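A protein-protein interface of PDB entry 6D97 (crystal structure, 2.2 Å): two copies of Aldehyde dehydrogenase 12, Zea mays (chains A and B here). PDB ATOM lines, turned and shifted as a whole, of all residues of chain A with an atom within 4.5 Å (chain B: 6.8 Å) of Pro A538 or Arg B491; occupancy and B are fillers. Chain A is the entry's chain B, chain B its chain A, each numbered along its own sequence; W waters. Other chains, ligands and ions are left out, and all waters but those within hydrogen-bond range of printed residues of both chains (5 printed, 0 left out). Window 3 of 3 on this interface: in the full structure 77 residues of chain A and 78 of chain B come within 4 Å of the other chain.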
ATOM      1  N   HIS A 177      30.667   9.007  10.175  1.00  0.00           N
ATOM      2  CA  HIS A 177      29.612   8.746   9.207  1.00  0.00           C
ATOM      3  C   HIS A 177      28.838  10.031   8.971  1.00  0.00           C
ATOM      4  O   HIS A 177      28.971  11.008   9.714  1.00  0.00           O
ATOM      5  CB  HIS A 177      28.671   7.633   9.681  1.00  0.00           C
ATOM      6  CG  HIS A 177      28.167   7.825  11.078  1.00  0.00           C
ATOM      7  ND1 HIS A 177      28.663   7.115  12.148  1.00  0.00           N
ATOM      8  CD2 HIS A 177      27.225   8.658  11.583  1.00  0.00           C
ATOM      9  CE1 HIS A 177      28.047   7.498  13.253  1.00  0.00           C
ATOM     10  NE2 HIS A 177      27.168   8.432  12.937  1.00  0.00           N
ATOM     11  N   ASP A 533      25.282  14.348  15.963  1.00  0.00           N
ATOM     12  CA  ASP A 533      25.034  13.027  15.373  1.00  0.00           C
ATOM     13  C   ASP A 533      23.550  13.008  14.989  1.00  0.00           C
ATOM     14  O   ASP A 533      22.697  12.437  15.674  1.00  0.00           O
ATOM     15  CB  ASP A 533      25.390  11.886  16.329  1.00  0.00           C
ATOM     16  CG  ASP A 533      25.978  10.687  15.606  1.00  0.00           C
ATOM     17  OD1 ASP A 533      25.715  10.545  14.391  1.00  0.00           O
ATOM     18  OD2 ASP A 533      26.712   9.901  16.244  1.00  0.00           O
ATOM     19  N   GLY A 535      21.981  11.926  12.138  1.00  0.00           N
ATOM     20  CA  GLY A 535      21.456  10.934  11.231  1.00  0.00           C
ATOM     21  C   GLY A 535      21.856  11.211   9.795  1.00  0.00           C
ATOM     22  O   GLY A 535      22.722  12.047   9.524  1.00  0.00           O
ATOM     23  N   PRO A 536      21.219  10.523   8.830  1.00  0.00           N
ATOM     24  CA  PRO A 536      20.137   9.541   8.972  1.00  0.00           C
ATOM     25  C   PRO A 536      20.564   8.253   9.661  1.00  0.00           C
ATOM     26  O   PRO A 536      21.732   7.878   9.575  1.00  0.00           O
ATOM     27  CB  PRO A 536      19.742   9.253   7.520  1.00  0.00           C
ATOM     28  CG  PRO A 536      20.983   9.553   6.738  1.00  0.00           C
ATOM     29  CD  PRO A 536      21.552  10.755   7.414  1.00  0.00           C
ATOM     30  N   VAL A 537      19.634   7.606  10.355  1.00  0.00           N
ATOM     31  CA  VAL A 537      19.852   6.242  10.822  1.00  0.00           C
ATOM     32  C   VAL A 537      20.036   5.392   9.572  1.00  0.00           C
ATOM     33  O   VAL A 537      19.149   5.376   8.706  1.00  0.00           O
ATOM     34  CB  VAL A 537      18.689   5.739  11.688  1.00  0.00           C
ATOM     35  CG1 VAL A 537      18.777   4.234  11.865  1.00  0.00           C
ATOM     36  CG2 VAL A 537      18.705   6.433  13.034  1.00  0.00           C
ATOM     37  N   PRO A 538      21.166   4.702   9.422  1.00  0.00           N
ATOM     38  CA  PRO A 538      21.480   4.083   8.131  1.00  0.00           C
ATOM     39  C   PRO A 538      20.423   3.087   7.685  1.00  0.00           C
ATOM     40  O   PRO A 538      19.708   2.489   8.493  1.00  0.00           O
ATOM     41  CB  PRO A 538      22.823   3.389   8.387  1.00  0.00           C
ATOM     42  CG  PRO A 538      23.439   4.172   9.497  1.00  0.00           C
ATOM     43  CD  PRO A 538      22.292   4.614  10.368  1.00  0.00           C
ATOM     44  N   GLU A 539      20.320   2.946   6.364  1.00  0.00           N
ATOM     45  CA  GLU A 539      19.515   1.892   5.760  1.00  0.00           C
ATOM     46  C   GLU A 539      19.886   0.525   6.323  1.00  0.00           C
ATOM     47  O   GLU A 539      19.007  -0.279   6.657  1.00  0.00           O
ATOM     48  CB  GLU A 539      19.718   1.938   4.244  1.00  0.00           C
ATOM     49  CG  GLU A 539      18.798   1.082   3.398  1.00  0.00           C
ATOM     50  CD  GLU A 539      19.145   1.195   1.923  1.00  0.00           C
ATOM     51  OE1 GLU A 539      18.928   2.281   1.341  1.00  0.00           O
ATOM     52  OE2 GLU A 539      19.669   0.212   1.357  1.00  0.00           O
ATOM     53  N   SER A 540      21.186   0.253   6.455  1.00  0.00           N
ATOM     54  CA  SER A 540      21.672  -1.044   6.909  1.00  0.00           C
ATOM     55  C   SER A 540      21.464  -1.282   8.396  1.00  0.00           C
ATOM     56  O   SER A 540      21.723  -2.398   8.861  1.00  0.00           O
ATOM     57  CB  SER A 540      23.164  -1.184   6.600  1.00  0.00           C
ATOM     58  OG  SER A 540      23.939  -0.382   7.479  1.00  0.00           O
ATOM     59  N   TRP A 541      21.036  -0.278   9.156  1.00  0.00           N
ATOM     60  CA  TRP A 541      20.987  -0.440  10.603  1.00  0.00           C
ATOM     61  C   TRP A 541      19.868  -1.391  10.994  1.00  0.00           C
ATOM     62  O   TRP A 541      18.685  -1.098  10.788  1.00  0.00           O
ATOM     63  CB  TRP A 541      20.805   0.898  11.312  1.00  0.00           C
ATOM     64  CG  TRP A 541      20.936   0.731  12.800  1.00  0.00           C
ATOM     65  CD1 TRP A 541      22.097   0.687  13.519  1.00  0.00           C
ATOM     66  CD2 TRP A 541      19.873   0.546  13.746  1.00  0.00           C
ATOM     67  NE1 TRP A 541      21.822   0.503  14.851  1.00  0.00           N
ATOM     68  CE2 TRP A 541      20.465   0.415  15.018  1.00  0.00           C
ATOM     69  CE3 TRP A 541      18.478   0.486  13.641  1.00  0.00           C
ATOM     70  CZ2 TRP A 541      19.713   0.224  16.177  1.00  0.00           C
ATOM     71  CZ3 TRP A 541      17.731   0.305  14.794  1.00  0.00           C
ATOM     72  CH2 TRP A 541      18.351   0.169  16.044  1.00  0.00           C
ATOM     73  N   GLU B 308      12.709   7.546  15.193  1.00  0.00           N
ATOM     74  CA  GLU B 308      13.722   6.495  15.311  1.00  0.00           C
ATOM     75  C   GLU B 308      13.677   5.843  16.691  1.00  0.00           C
ATOM     76  O   GLU B 308      14.697   5.683  17.364  1.00  0.00           O
ATOM     77  CB  GLU B 308      15.122   7.037  15.011  1.00  0.00           C
ATOM     78  CG  GLU B 308      15.258   7.741  13.672  1.00  0.00           C
ATOM     79  CD  GLU B 308      15.176   6.787  12.492  1.00  0.00           C
ATOM     80  OE1 GLU B 308      15.110   7.275  11.343  1.00  0.00           O
ATOM     81  OE2 GLU B 308      15.179   5.555  12.707  1.00  0.00           O
ATOM     82  N   TYR B 311      16.021   2.900  17.311  1.00  0.00           N
ATOM     83  CA  TYR B 311      17.417   3.301  17.443  1.00  0.00           C
ATOM     84  C   TYR B 311      17.673   3.983  18.780  1.00  0.00           C
ATOM     85  O   TYR B 311      18.675   3.701  19.447  1.00  0.00           O
ATOM     86  CB  TYR B 311      17.818   4.226  16.293  1.00  0.00           C
ATOM     87  CG  TYR B 311      19.308   4.501  16.241  1.00  0.00           C
ATOM     88  CD1 TYR B 311      19.885   5.488  17.033  1.00  0.00           C
ATOM     89  CD2 TYR B 311      20.138   3.766  15.403  1.00  0.00           C
ATOM     90  CE1 TYR B 311      21.246   5.734  16.991  1.00  0.00           C
ATOM     91  CE2 TYR B 311      21.498   4.007  15.352  1.00  0.00           C
ATOM     92  CZ  TYR B 311      22.046   4.990  16.149  1.00  0.00           C
ATOM     93  OH  TYR B 311      23.400   5.230  16.101  1.00  0.00           O
ATOM     94  N   VAL B 312      16.782   4.895  19.180  1.00  0.00           N
ATOM     95  CA  VAL B 312      16.957   5.615  20.438  1.00  0.00           C
ATOM     96  C   VAL B 312      16.908   4.652  21.618  1.00  0.00           C
ATOM     97  O   VAL B 312      17.674   4.786  22.579  1.00  0.00           O
ATOM     98  CB  VAL B 312      15.898   6.727  20.568  1.00  0.00           C
ATOM     99  CG1 VAL B 312      15.967   7.376  21.942  1.00  0.00           C
ATOM    100  CG2 VAL B 312      16.096   7.764  19.474  1.00  0.00           C
ATOM    101  N   TRP B 314      17.751   1.444  21.639  1.00  0.00           N
ATOM    102  CA  TRP B 314      18.990   0.674  21.655  1.00  0.00           C
ATOM    103  C   TRP B 314      20.122   1.470  22.287  1.00  0.00           C
ATOM    104  O   TRP B 314      20.889   0.943  23.103  1.00  0.00           O
ATOM    105  CB  TRP B 314      19.352   0.253  20.232  1.00  0.00           C
ATOM    106  CG  TRP B 314      20.734  -0.297  20.071  1.00  0.00           C
ATOM    107  CD1 TRP B 314      21.197  -1.506  20.503  1.00  0.00           C
ATOM    108  CD2 TRP B 314      21.828   0.336  19.399  1.00  0.00           C
ATOM    109  NE1 TRP B 314      22.517  -1.660  20.150  1.00  0.00           N
ATOM    110  CE2 TRP B 314      22.927  -0.542  19.472  1.00  0.00           C
ATOM    111  CE3 TRP B 314      21.986   1.560  18.742  1.00  0.00           C
ATOM    112  CZ2 TRP B 314      24.166  -0.233  18.914  1.00  0.00           C
ATOM    113  CZ3 TRP B 314      23.216   1.866  18.188  1.00  0.00           C
ATOM    114  CH2 TRP B 314      24.289   0.973  18.278  1.00  0.00           C
ATOM    115  N   VAL B 315      20.230   2.751  21.934  1.00  0.00           N
ATOM    116  CA  VAL B 315      21.286   3.585  22.496  1.00  0.00           C
ATOM    117  C   VAL B 315      21.071   3.784  23.988  1.00  0.00           C
ATOM    118  O   VAL B 315      22.029   3.808  24.771  1.00  0.00           O
ATOM    119  CB  VAL B 315      21.354   4.927  21.748  1.00  0.00           C
ATOM    120  CG1 VAL B 315      22.375   5.835  22.393  1.00  0.00           C
ATOM    121  CG2 VAL B 315      21.695   4.691  20.295  1.00  0.00           C
ATOM    122  N   ILE B 466      21.536  14.944  24.042  1.00  0.00           N
ATOM    123  CA  ILE B 466      20.304  15.658  23.731  1.00  0.00           C
ATOM    124  C   ILE B 466      19.742  14.999  22.480  1.00  0.00           C
ATOM    125  O   ILE B 466      20.217  15.248  21.364  1.00  0.00           O
ATOM    126  CB  ILE B 466      20.533  17.157  23.523  1.00  0.00           C
ATOM    127  CG1 ILE B 466      21.454  17.707  24.615  1.00  0.00           C
ATOM    128  CG2 ILE B 466      19.199  17.897  23.526  1.00  0.00           C
ATOM    129  CD1 ILE B 466      22.111  19.002  24.248  1.00  0.00           C
ATOM    130  N   VAL B 467      18.736  14.146  22.660  1.00  0.00           N
ATOM    131  CA  VAL B 467      18.184  13.348  21.566  1.00  0.00           C
ATOM    132  C   VAL B 467      17.073  14.178  20.929  1.00  0.00           C
ATOM    133  O   VAL B 467      15.919  14.160  21.359  1.00  0.00           O
ATOM    134  CB  VAL B 467      17.695  11.985  22.044  1.00  0.00           C
ATOM    135  CG1 VAL B 467      17.154  11.184  20.873  1.00  0.00           C
ATOM    136  CG2 VAL B 467      18.826  11.237  22.742  1.00  0.00           C
ATOM    137  N   SER B 468      17.440  14.912  19.881  1.00  0.00           N
ATOM    138  CA  SER B 468      16.552  15.769  19.109  1.00  0.00           C
ATOM    139  C   SER B 468      17.318  16.248  17.888  1.00  0.00           C
ATOM    140  O   SER B 468      18.543  16.395  17.932  1.00  0.00           O
ATOM    141  CB  SER B 468      16.062  16.969  19.931  1.00  0.00           C
ATOM    142  OG  SER B 468      15.479  17.958  19.100  1.00  0.00           O
ATOM    143  N   ASN B 469      16.591  16.476  16.795  1.00  0.00           N
ATOM    144  CA  ASN B 469      17.156  17.092  15.601  1.00  0.00           C
ATOM    145  C   ASN B 469      16.656  18.511  15.380  1.00  0.00           C
ATOM    146  O   ASN B 469      17.046  19.144  14.394  1.00  0.00           O
ATOM    147  CB  ASN B 469      16.861  16.238  14.364  1.00  0.00           C
ATOM    148  CG  ASN B 469      17.939  15.212  14.109  1.00  0.00           C
ATOM    149  OD1 ASN B 469      18.859  15.059  14.908  1.00  0.00           O
ATOM    150  ND2 ASN B 469      17.835  14.503  12.995  1.00  0.00           N
ATOM    151  N   TYR B 487      26.688  15.092  23.414  1.00  0.00           N
ATOM    152  CA  TYR B 487      26.265  14.651  22.092  1.00  0.00           C
ATOM    153  C   TYR B 487      24.870  15.192  21.805  1.00  0.00           C
ATOM    154  O   TYR B 487      24.010  15.216  22.690  1.00  0.00           O
ATOM    155  CB  TYR B 487      26.272  13.124  21.988  1.00  0.00           C
ATOM    156  CG  TYR B 487      27.612  12.470  22.265  1.00  0.00           C
ATOM    157  CD1 TYR B 487      28.103  12.364  23.561  1.00  0.00           C
ATOM    158  CD2 TYR B 487      28.374  11.940  21.231  1.00  0.00           C
ATOM    159  CE1 TYR B 487      29.315  11.758  23.822  1.00  0.00           C
ATOM    160  CE2 TYR B 487      29.595  11.339  21.482  1.00  0.00           C
ATOM    161  CZ  TYR B 487      30.059  11.251  22.778  1.00  0.00           C
ATOM    162  OH  TYR B 487      31.269  10.646  23.029  1.00  0.00           O
ATOM    163  N   ALA B 488      24.647  15.625  20.565  1.00  0.00           N
ATOM    164  CA  ALA B 488      23.398  16.278  20.188  1.00  0.00           C
ATOM    165  C   ALA B 488      22.946  15.770  18.829  1.00  0.00           C
ATOM    166  O   ALA B 488      23.727  15.766  17.874  1.00  0.00           O
ATOM    167  CB  ALA B 488      23.556  17.803  20.156  1.00  0.00           C
ATOM    168  N   GLY B 489      21.684  15.367  18.742  1.00  0.00           N
ATOM    169  CA  GLY B 489      21.151  14.785  17.529  1.00  0.00           C
ATOM    170  C   GLY B 489      20.280  13.600  17.874  1.00  0.00           C
ATOM    171  O   GLY B 489      20.288  13.149  19.023  1.00  0.00           O
ATOM    172  N   ILE B 490      19.517  13.084  16.909  1.00  0.00           N
ATOM    173  CA  ILE B 490      18.652  11.948  17.207  1.00  0.00           C
ATOM    174  C   ILE B 490      19.467  10.701  17.524  1.00  0.00           C
ATOM    175  O   ILE B 490      18.962   9.787  18.186  1.00  0.00           O
ATOM    176  CB  ILE B 490      17.668  11.695  16.049  1.00  0.00           C
ATOM    177  CG1 ILE B 490      16.401  11.010  16.568  1.00  0.00           C
ATOM    178  CG2 ILE B 490      18.314  10.858  14.955  1.00  0.00           C
ATOM    179  CD1 ILE B 490      15.625  11.841  17.586  1.00  0.00           C
ATOM    180  N   ARG B 491      20.726  10.644  17.084  1.00  0.00           N
ATOM    181  CA  ARG B 491      21.616   9.530  17.381  1.00  0.00           C
ATOM    182  C   ARG B 491      22.535   9.823  18.559  1.00  0.00           C
ATOM    183  O   ARG B 491      23.553   9.140  18.728  1.00  0.00           O
ATOM    184  CB  ARG B 491      22.438   9.169  16.140  1.00  0.00           C
ATOM    185  CG  ARG B 491      21.591   8.719  14.956  1.00  0.00           C
ATOM    186  CD  ARG B 491      22.440   8.401  13.735  1.00  0.00           C
ATOM    187  NE  ARG B 491      23.297   7.235  13.936  1.00  0.00           N
ATOM    188  CZ  ARG B 491      24.069   6.708  12.992  1.00  0.00           C
ATOM    189  NH1 ARG B 491      24.095   7.242  11.778  1.00  0.00           N
ATOM    190  NH2 ARG B 491      24.816   5.646  13.263  1.00  0.00           N
ATOM    191  N   ALA B 492      22.196  10.818  19.379  1.00  0.00           N
ATOM    192  CA  ALA B 492      23.053  11.195  20.495  1.00  0.00           C
ATOM    193  C   ALA B 492      23.115  10.083  21.536  1.00  0.00           C
ATOM    194  O   ALA B 492      22.128   9.388  21.795  1.00  0.00           O
ATOM    195  CB  ALA B 492      22.554  12.491  21.139  1.00  0.00           C
ATOM    196  N   ARG B 493      24.294   9.928  22.130  1.00  0.00           N
ATOM    197  CA  ARG B 493      24.572   8.929  23.149  1.00  0.00           C
ATOM    198  C   ARG B 493      25.311   9.601  24.299  1.00  0.00           C
ATOM    199  O   ARG B 493      25.720  10.759  24.205  1.00  0.00           O
ATOM    200  CB  ARG B 493      25.409   7.781  22.569  1.00  0.00           C
ATOM    201  CG  ARG B 493      26.767   8.230  22.025  1.00  0.00           C
ATOM    202  CD  ARG B 493      27.391   7.191  21.109  1.00  0.00           C
ATOM    203  NE  ARG B 493      28.838   7.362  21.019  1.00  0.00           N
ATOM    204  CZ  ARG B 493      29.452   8.137  20.132  1.00  0.00           C
ATOM    205  NH1 ARG B 493      28.745   8.815  19.238  1.00  0.00           N
ATOM    206  NH2 ARG B 493      30.776   8.230  20.139  1.00  0.00           N
HETATM  207  O   HOH W   1      26.170   7.246  16.268  1.00  0.00           O
HETATM  208  O   HOH W   2      24.344   8.318   8.805  1.00  0.00           O
HETATM  209  O   HOH W   3      26.330   9.682  19.058  1.00  0.00           O
HETATM  210  O   HOH W   4      24.559  10.677  11.972  1.00  0.00           O
HETATM  211  O   HOH W   5      17.168   8.819  10.357  1.00  0.00           O
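The backbone carbonyl oxygen (O) of Ala B488 sits at hydrogen-bond distance from the backbone NH (N) of Asp A533 (2.8 Å).
The backbone NH (N) of Ile B490 sits at hydrogen-bond distance from the backbone carbonyl oxygen (O) of Asp A533 (3.5 Å).
A ring nitrogen (NE2) of His A177 lies close to the guanidinium group of Arg B491.
The backbone NH (N) of Arg B491 sits at hydrogen-bond distance from the backbone carbonyl oxygen (O) of Asp A533, at 3.0 Å.
O of Pro A536 is in hydrogen-bond range of NH1 of Arg B491, at 3.3 Å.
NH1 of Arg B493 lies within salt-bridge range of OD2 of Asp A533 (3.8 Å).
OH of Tyr B311 is in hydrogen-bond range of NE of Arg B491, 3.0 Å away.
O of Ile B466 is in hydrogen-bond range of N of Gly B489 (3.0 Å).
The backbone carbonyl oxygen (O) of Ser B468 lies close to the backbone NH (N) of Gly B489.
The side-chain amide oxygen of Asn B469 is in hydrogen-bond range of the backbone NH of Ile B490.
NE2 of His A177 lies within hydrogen-bond range of OD1 of Asp A533 (2.9 Å).
Among the printed residues, pairs that only touch across the chains: Asp A533 with Gly B489, Gly A535 with Arg B491, Val A537 with Glu B308, Val A537 with Tyr B311, Pro A538 with Arg B491, Trp A541 with Tyr B311 and Trp A541 with Trp B314.
Printed residues of chain B within 4 Å of Asp A533: Ala B488, Gly B489, Ile B490, Arg B491 and Arg B493.
Of the printed residues of chain B, Pro A536 touches Arg B491 (3.3 Å).
Of chain B, only Arg B491 comes within 4 Å of Pro A538.
Printed residues of chain B within 4 Å of Trp A541: Tyr B311 and Trp B314.
Ile B466 touches none of the printed residues of chain A.
Printed residues of chain A within 4 Å of Gly B489: Asp A533.
The nearest residue of chain B that does not touch Pro A538 is Tyr B311 (5.1 Å).
Hydrophobic or aromatic side chains of chain B that line the printed part of chain A: Tyr B311 and Trp B314.
Printed residues of chain A that touch a printed residue of chain B: His A177, Asp A533, Gly A535, Pro A536, Val A537, Pro A538 and Trp A541.
Hydrophobic or aromatic side chains of chain A within 4 Å of the printed part of chain B: His A177, Val A537, Pro A538 and Trp A541.
Among the printed residues, Asp or Glu carboxylates within 4 Å of a Lys or Arg side-chain nitrogen of the other chain: Asp A533 with Arg B493 (3.8 Å).
No position is printed for both chains.
Water W3 lies within hydrogen-bond range of the guanidinium group of Arg B493 (2.6 Å), the side-chain carboxylate of Asp A533 (2.8 Å) and the backbone carbonyl oxygen of Arg B491 (2.8 Å).
Water W4 lies within hydrogen-bond range of the side-chain carboxylate (OD1) of Asp A533 (2.7 Å), the backbone NH (N) of Gly A535 (2.9 Å) and the guanidinium group (NH1) of Arg B491 (3.5 Å).
Water W1 bridges the side-chain carboxylate of Asp A533 (2.7 Å) and the side-chain hydroxyl of Tyr B311 (3.4 Å).
Water W5 lies within hydrogen-bond range of N of Val A537 (2.7 Å) and OE1 of Glu B308 (2.8 Å).
Water W2 lies within hydrogen-bond range of O of Pro A536 (2.8 Å) and NH1 of Arg B491 (3.2 Å).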
